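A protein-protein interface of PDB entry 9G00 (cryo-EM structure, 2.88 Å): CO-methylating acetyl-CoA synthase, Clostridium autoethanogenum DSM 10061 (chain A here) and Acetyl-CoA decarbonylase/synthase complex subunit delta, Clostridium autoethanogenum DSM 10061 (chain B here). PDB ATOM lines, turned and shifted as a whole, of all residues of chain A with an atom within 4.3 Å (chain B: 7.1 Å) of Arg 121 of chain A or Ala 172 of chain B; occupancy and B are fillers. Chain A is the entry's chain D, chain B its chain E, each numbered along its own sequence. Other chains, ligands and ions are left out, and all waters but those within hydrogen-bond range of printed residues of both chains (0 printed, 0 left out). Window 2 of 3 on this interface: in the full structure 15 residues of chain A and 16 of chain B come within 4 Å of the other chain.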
ATOM      1  N   ASP A 117     -14.603  30.628  12.252  1.00  0.00           N
ATOM      2  CA  ASP A 117     -13.861  29.395  12.020  1.00  0.00           C
ATOM      3  C   ASP A 117     -14.482  28.166  12.668  1.00  0.00           C
ATOM      4  O   ASP A 117     -14.483  27.097  12.024  1.00  0.00           O
ATOM      5  CB  ASP A 117     -12.419  29.559  12.511  1.00  0.00           C
ATOM      6  CG  ASP A 117     -11.481  30.077  11.435  1.00  0.00           C
ATOM      7  OD1 ASP A 117     -11.713  29.756  10.254  1.00  0.00           O
ATOM      8  OD2 ASP A 117     -10.517  30.790  11.765  1.00  0.00           O
ATOM      9  N   PRO A 118     -14.958  28.208  13.918  1.00  0.00           N
ATOM     10  CA  PRO A 118     -15.572  26.990  14.474  1.00  0.00           C
ATOM     11  C   PRO A 118     -16.745  26.489  13.658  1.00  0.00           C
ATOM     12  O   PRO A 118     -16.946  25.275  13.559  1.00  0.00           O
ATOM     13  CB  PRO A 118     -15.988  27.420  15.887  1.00  0.00           C
ATOM     14  CG  PRO A 118     -15.033  28.563  16.234  1.00  0.00           C
ATOM     15  CD  PRO A 118     -14.808  29.276  14.921  1.00  0.00           C
ATOM     16  N   ILE A 119     -17.512  27.387  13.038  1.00  0.00           N
ATOM     17  CA  ILE A 119     -18.603  26.948  12.173  1.00  0.00           C
ATOM     18  C   ILE A 119     -18.045  26.206  10.969  1.00  0.00           C
ATOM     19  O   ILE A 119     -18.579  25.171  10.551  1.00  0.00           O
ATOM     20  CB  ILE A 119     -19.481  28.139  11.762  1.00  0.00           C
ATOM     21  CG1 ILE A 119     -20.235  28.658  12.995  1.00  0.00           C
ATOM     22  CG2 ILE A 119     -20.446  27.737  10.644  1.00  0.00           C
ATOM     23  CD1 ILE A 119     -21.095  29.880  12.725  1.00  0.00           C
ATOM     24  N   ILE A 120     -16.961  26.735  10.392  1.00  0.00           N
ATOM     25  CA  ILE A 120     -16.374  26.067   9.228  1.00  0.00           C
ATOM     26  C   ILE A 120     -15.908  24.666   9.590  1.00  0.00           C
ATOM     27  O   ILE A 120     -16.119  23.720   8.837  1.00  0.00           O
ATOM     28  CB  ILE A 120     -15.240  26.905   8.624  1.00  0.00           C
ATOM     29  CG1 ILE A 120     -15.834  28.189   8.028  1.00  0.00           C
ATOM     30  CG2 ILE A 120     -14.464  26.095   7.564  1.00  0.00           C
ATOM     31  CD1 ILE A 120     -14.835  29.030   7.269  1.00  0.00           C
ATOM     32  N   ARG A 121     -15.237  24.520  10.728  1.00  0.00           N
ATOM     33  CA  ARG A 121     -14.836  23.182  11.177  1.00  0.00           C
ATOM     34  C   ARG A 121     -16.046  22.305  11.488  1.00  0.00           C
ATOM     35  O   ARG A 121     -15.986  21.081  11.324  1.00  0.00           O
ATOM     36  CB  ARG A 121     -13.935  23.281  12.408  1.00  0.00           C
ATOM     37  CG  ARG A 121     -12.698  24.140  12.189  1.00  0.00           C
ATOM     38  CD  ARG A 121     -11.831  24.170  13.450  1.00  0.00           C
ATOM     39  NE  ARG A 121     -10.788  25.185  13.366  1.00  0.00           N
ATOM     40  CZ  ARG A 121      -9.578  24.988  12.857  1.00  0.00           C
ATOM     41  NH1 ARG A 121      -9.197  23.803  12.410  1.00  0.00           N
ATOM     42  NH2 ARG A 121      -8.725  26.012  12.789  1.00  0.00           N
ATOM     43  N   SER A 122     -17.144  22.908  11.936  1.00  0.00           N
ATOM     44  CA  SER A 122     -18.361  22.149  12.204  1.00  0.00           C
ATOM     45  C   SER A 122     -18.955  21.560  10.930  1.00  0.00           C
ATOM     46  O   SER A 122     -19.341  20.387  10.908  1.00  0.00           O
ATOM     47  CB  SER A 122     -19.372  23.064  12.904  1.00  0.00           C
ATOM     48  OG  SER A 122     -20.600  22.393  13.163  1.00  0.00           O
ATOM     49  N   LEU A 123     -19.026  22.343   9.863  1.00  0.00           N
ATOM     50  CA  LEU A 123     -19.580  21.864   8.593  1.00  0.00           C
ATOM     51  C   LEU A 123     -18.521  21.325   7.637  1.00  0.00           C
ATOM     52  O   LEU A 123     -18.865  20.876   6.540  1.00  0.00           O
ATOM     53  CB  LEU A 123     -20.396  22.974   7.905  1.00  0.00           C
ATOM     54  CG  LEU A 123     -19.730  24.340   7.686  1.00  0.00           C
ATOM     55  CD1 LEU A 123     -18.843  24.359   6.447  1.00  0.00           C
ATOM     56  CD2 LEU A 123     -20.804  25.418   7.604  1.00  0.00           C
ATOM     57  N   GLY A 124     -17.247  21.372   8.017  1.00  0.00           N
ATOM     58  CA  GLY A 124     -16.205  20.842   7.160  1.00  0.00           C
ATOM     59  C   GLY A 124     -16.256  19.334   7.018  1.00  0.00           C
ATOM     60  O   GLY A 124     -16.002  18.796   5.939  1.00  0.00           O
ATOM     61  N   VAL A 125     -16.561  18.630   8.105  1.00  0.00           N
ATOM     62  CA  VAL A 125     -16.650  17.171   8.037  1.00  0.00           C
ATOM     63  C   VAL A 125     -17.754  16.725   7.085  1.00  0.00           C
ATOM     64  O   VAL A 125     -17.499  15.840   6.245  1.00  0.00           O
ATOM     65  CB  VAL A 125     -16.804  16.582   9.453  1.00  0.00           C
ATOM     66  CG1 VAL A 125     -16.541  15.079   9.429  1.00  0.00           C
ATOM     67  CG2 VAL A 125     -15.856  17.278  10.441  1.00  0.00           C
ATOM     68  N   ILE A 208      -7.692  25.406   6.160  1.00  0.00           N
ATOM     69  CA  ILE A 208      -7.851  24.512   7.304  1.00  0.00           C
ATOM     70  C   ILE A 208      -7.720  23.056   6.896  1.00  0.00           C
ATOM     71  O   ILE A 208      -6.934  22.306   7.480  1.00  0.00           O
ATOM     72  CB  ILE A 208      -9.209  24.785   7.989  1.00  0.00           C
ATOM     73  CG1 ILE A 208      -9.242  26.215   8.546  1.00  0.00           C
ATOM     74  CG2 ILE A 208      -9.462  23.766   9.103  1.00  0.00           C
ATOM     75  CD1 ILE A 208     -10.575  26.622   9.166  1.00  0.00           C
ATOM     76  N   PHE A 209      -8.493  22.611   5.905  1.00  0.00           N
ATOM     77  CA  PHE A 209      -8.500  21.203   5.530  1.00  0.00           C
ATOM     78  C   PHE A 209      -7.458  20.872   4.472  1.00  0.00           C
ATOM     79  O   PHE A 209      -6.885  19.779   4.503  1.00  0.00           O
ATOM     80  CB  PHE A 209      -9.894  20.799   5.039  1.00  0.00           C
ATOM     81  CG  PHE A 209     -11.002  21.247   5.948  1.00  0.00           C
ATOM     82  CD1 PHE A 209     -11.152  20.675   7.210  1.00  0.00           C
ATOM     83  CD2 PHE A 209     -11.879  22.251   5.560  1.00  0.00           C
ATOM     84  CE1 PHE A 209     -12.167  21.092   8.078  1.00  0.00           C
ATOM     85  CE2 PHE A 209     -12.901  22.686   6.414  1.00  0.00           C
ATOM     86  CZ  PHE A 209     -13.040  22.105   7.681  1.00  0.00           C
ATOM     87  N   GLU B 141     -16.668  11.904  15.543  1.00  0.00           N
ATOM     88  CA  GLU B 141     -16.961  13.284  15.173  1.00  0.00           C
ATOM     89  C   GLU B 141     -17.209  14.133  16.411  1.00  0.00           C
ATOM     90  O   GLU B 141     -16.727  15.269  16.502  1.00  0.00           O
ATOM     91  CB  GLU B 141     -18.168  13.337  14.238  1.00  0.00           C
ATOM     92  CG  GLU B 141     -18.528  14.742  13.779  1.00  0.00           C
ATOM     93  CD  GLU B 141     -19.721  14.766  12.843  1.00  0.00           C
ATOM     94  OE1 GLU B 141     -20.204  13.678  12.467  1.00  0.00           O
ATOM     95  OE2 GLU B 141     -20.176  15.872  12.486  1.00  0.00           O
ATOM     96  N   ALA B 144     -13.760  14.115  18.862  1.00  0.00           N
ATOM     97  CA  ALA B 144     -12.688  15.001  18.421  1.00  0.00           C
ATOM     98  C   ALA B 144     -13.063  16.464  18.603  1.00  0.00           C
ATOM     99  O   ALA B 144     -12.176  17.313  18.752  1.00  0.00           O
ATOM    100  CB  ALA B 144     -12.346  14.718  16.960  1.00  0.00           C
ATOM    101  N   GLU B 148     -10.502  19.067  21.863  1.00  0.00           N
ATOM    102  CA  GLU B 148      -9.767  19.842  20.875  1.00  0.00           C
ATOM    103  C   GLU B 148      -8.631  20.583  21.563  1.00  0.00           C
ATOM    104  O   GLU B 148      -8.837  21.205  22.612  1.00  0.00           O
ATOM    105  CB  GLU B 148     -10.682  20.833  20.156  1.00  0.00           C
ATOM    106  CG  GLU B 148      -9.973  21.642  19.083  1.00  0.00           C
ATOM    107  CD  GLU B 148     -10.895  22.604  18.372  1.00  0.00           C
ATOM    108  OE1 GLU B 148     -12.069  22.711  18.780  1.00  0.00           O
ATOM    109  OE2 GLU B 148     -10.447  23.251  17.403  1.00  0.00           O
ATOM    110  N   GLY B 166     -11.375  10.422   9.466  1.00  0.00           N
ATOM    111  CA  GLY B 166     -10.225  11.217   9.068  1.00  0.00           C
ATOM    112  C   GLY B 166     -10.534  12.700   8.986  1.00  0.00           C
ATOM    113  O   GLY B 166      -9.735  13.533   9.417  1.00  0.00           O
ATOM    114  N   ALA B 167     -11.694  13.049   8.428  1.00  0.00           N
ATOM    115  CA  ALA B 167     -12.068  14.456   8.315  1.00  0.00           C
ATOM    116  C   ALA B 167     -12.307  15.074   9.687  1.00  0.00           C
ATOM    117  O   ALA B 167     -11.764  16.138  10.002  1.00  0.00           O
ATOM    118  CB  ALA B 167     -13.309  14.597   7.436  1.00  0.00           C
ATOM    119  N   ALA B 168     -13.120  14.421  10.517  1.00  0.00           N
ATOM    120  CA  ALA B 168     -13.367  14.911  11.867  1.00  0.00           C
ATOM    121  C   ALA B 168     -12.154  14.758  12.770  1.00  0.00           C
ATOM    122  O   ALA B 168     -12.151  15.307  13.877  1.00  0.00           O
ATOM    123  CB  ALA B 168     -14.553  14.179  12.486  1.00  0.00           C
ATOM    124  N   GLY B 169     -11.134  14.039  12.323  1.00  0.00           N
ATOM    125  CA  GLY B 169      -9.938  13.807  13.100  1.00  0.00           C
ATOM    126  C   GLY B 169      -8.808  14.708  12.660  1.00  0.00           C
ATOM    127  O   GLY B 169      -8.709  15.854  13.105  1.00  0.00           O
ATOM    128  N   VAL B 170      -7.947  14.193  11.784  1.00  0.00           N
ATOM    129  CA  VAL B 170      -6.722  14.901  11.423  1.00  0.00           C
ATOM    130  C   VAL B 170      -7.028  16.295  10.889  1.00  0.00           C
ATOM    131  O   VAL B 170      -6.466  17.292  11.355  1.00  0.00           O
ATOM    132  CB  VAL B 170      -5.930  14.083  10.389  1.00  0.00           C
ATOM    133  CG1 VAL B 170      -4.904  14.949   9.690  1.00  0.00           C
ATOM    134  CG2 VAL B 170      -5.254  12.910  11.049  1.00  0.00           C
ATOM    135  N   MET B 171      -7.925  16.388   9.909  1.00  0.00           N
ATOM    136  CA  MET B 171      -8.049  17.632   9.153  1.00  0.00           C
ATOM    137  C   MET B 171      -8.757  18.721   9.947  1.00  0.00           C
ATOM    138  O   MET B 171      -8.330  19.882   9.931  1.00  0.00           O
ATOM    139  CB  MET B 171      -8.784  17.374   7.839  1.00  0.00           C
ATOM    140  CG  MET B 171      -8.049  16.429   6.906  1.00  0.00           C
ATOM    141  SD  MET B 171      -8.677  16.479   5.218  1.00  0.00           S
ATOM    142  CE  MET B 171     -10.418  16.171   5.486  1.00  0.00           C
ATOM    143  N   ALA B 172      -9.824  18.375  10.663  1.00  0.00           N
ATOM    144  CA  ALA B 172     -10.652  19.401  11.288  1.00  0.00           C
ATOM    145  C   ALA B 172     -10.040  19.905  12.589  1.00  0.00           C
ATOM    146  O   ALA B 172      -9.705  21.089  12.711  1.00  0.00           O
ATOM    147  CB  ALA B 172     -12.060  18.857  11.537  1.00  0.00           C
ATOM    148  N   TYR B 173      -9.878  19.023  13.570  1.00  0.00           N
ATOM    149  CA  TYR B 173      -9.459  19.413  14.907  1.00  0.00           C
ATOM    150  C   TYR B 173      -7.996  19.102  15.188  1.00  0.00           C
ATOM    151  O   TYR B 173      -7.569  19.170  16.343  1.00  0.00           O
ATOM    152  CB  TYR B 173     -10.357  18.745  15.945  1.00  0.00           C
ATOM    153  CG  TYR B 173     -11.814  19.093  15.756  1.00  0.00           C
ATOM    154  CD1 TYR B 173     -12.338  20.272  16.263  1.00  0.00           C
ATOM    155  CD2 TYR B 173     -12.660  18.252  15.052  1.00  0.00           C
ATOM    156  CE1 TYR B 173     -13.666  20.597  16.084  1.00  0.00           C
ATOM    157  CE2 TYR B 173     -13.987  18.569  14.868  1.00  0.00           C
ATOM    158  CZ  TYR B 173     -14.486  19.741  15.386  1.00  0.00           C
ATOM    159  OH  TYR B 173     -15.812  20.056  15.203  1.00  0.00           O
ATOM    160  N   ASN B 174      -7.219  18.767  14.158  1.00  0.00           N
ATOM    161  CA  ASN B 174      -5.772  18.614  14.287  1.00  0.00           C
ATOM    162  C   ASN B 174      -5.414  17.551  15.328  1.00  0.00           C
ATOM    163  O   ASN B 174      -4.698  17.796  16.298  1.00  0.00           O
ATOM    164  CB  ASN B 174      -5.127  19.964  14.619  1.00  0.00           C
ATOM    165  CG  ASN B 174      -3.788  20.149  13.942  1.00  0.00           C
ATOM    166  OD1 ASN B 174      -2.753  19.739  14.465  1.00  0.00           O
ATOM    167  ND2 ASN B 174      -3.800  20.768  12.766  1.00  0.00           N
ATOM    168  N   ASP B 175      -5.937  16.353  15.104  1.00  0.00           N
ATOM    169  CA  ASP B 175      -5.650  15.181  15.912  1.00  0.00           C
ATOM    170  C   ASP B 175      -4.895  14.164  15.063  1.00  0.00           C
ATOM    171  O   ASP B 175      -4.486  14.447  13.931  1.00  0.00           O
ATOM    172  CB  ASP B 175      -6.948  14.594  16.472  1.00  0.00           C
ATOM    173  CG  ASP B 175      -7.577  15.475  17.526  1.00  0.00           C
ATOM    174  OD1 ASP B 175      -6.942  16.471  17.926  1.00  0.00           O
ATOM    175  OD2 ASP B 175      -8.709  15.172  17.953  1.00  0.00           O
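CB of Ala 167 of chain B touches CG1 of Val 125 of chain A (3.8 Å). CG1 of Val 125 of chain A touches N of Ala 168 of chain B, at 3.6 Å. O of Met 171 of chain B touches O of Ile 208 of chain A, 3.7 Å away. Phe 209 of chain A touches Met 171 of chain B (O to SD, 3.8 Å). Phe 209 of chain A touches Ala 172 of chain B.
Of the 13 printed residues of chain B, 4 touch a printed residue of chain A. Of the 11 printed residues of chain A, 4 touch a printed residue of chain B. Printed residues of chain A that touch a printed residue of chain B: Arg 121, Val 125, Ile 208 and Phe 209. Hydrophobic or aromatic side chains of chain A within 4 Å of the printed part of chain B: Val 125 and Phe 209. Among the printed residues, no Asp or Glu carboxylate lies within 4 Å of a Lys or Arg side-chain nitrogen of the other chain.
N of Ala 172 of chain B lies within hydrogen-bond range of O of Ala 167 of chain B, 3.0 Å away. The backbone carbonyl oxygen (O) of Gly 166 of chain B is in hydrogen-bond range of the backbone NH (N) of Met 171 of chain B.
Of the printed residues of chain B, Arg 121 of chain A touches Ala 172. Of the printed residues of chain B, Ile 208 of chain A touches Met 171 (3.7 Å). Printed residues of chain B within 4 Å of Phe 209 of chain A: Met 171 (3.8 Å) and Ala 172 (3.9 Å). Gly 166 of chain B touches none of the printed residues of chain A. Of the printed residues of chain A, Ala 167 of chain B touches Val 125. Printed residues of chain A within 4 Å of Ala 168 of chain B: Val 125. Of the printed residues of chain A, Met 171 of chain B touches Ile 208 (3.7 Å) and Phe 209 (3.8 Å). Ala 172 of chain B touches just these residues of chain A: Arg 121 (2.8 Å) and Phe 209 (3.9 Å). Asp 175 of chain B touches none of the printed residues of chain A. The nearest printed residue of chain A that does not touch Ala 172 of chain B is Val 125 of chain A (4.3 Å). The nearest printed residue of chain A that does not touch Ala 168 of chain B is Arg 121 of chain A (6.7 Å).
The guanidinium group (NH1) of Arg 121 of chain A lies within hydrogen-bond range of the backbone carbonyl oxygen (O) of Ala 172 of chain B, 2.8 Å away.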
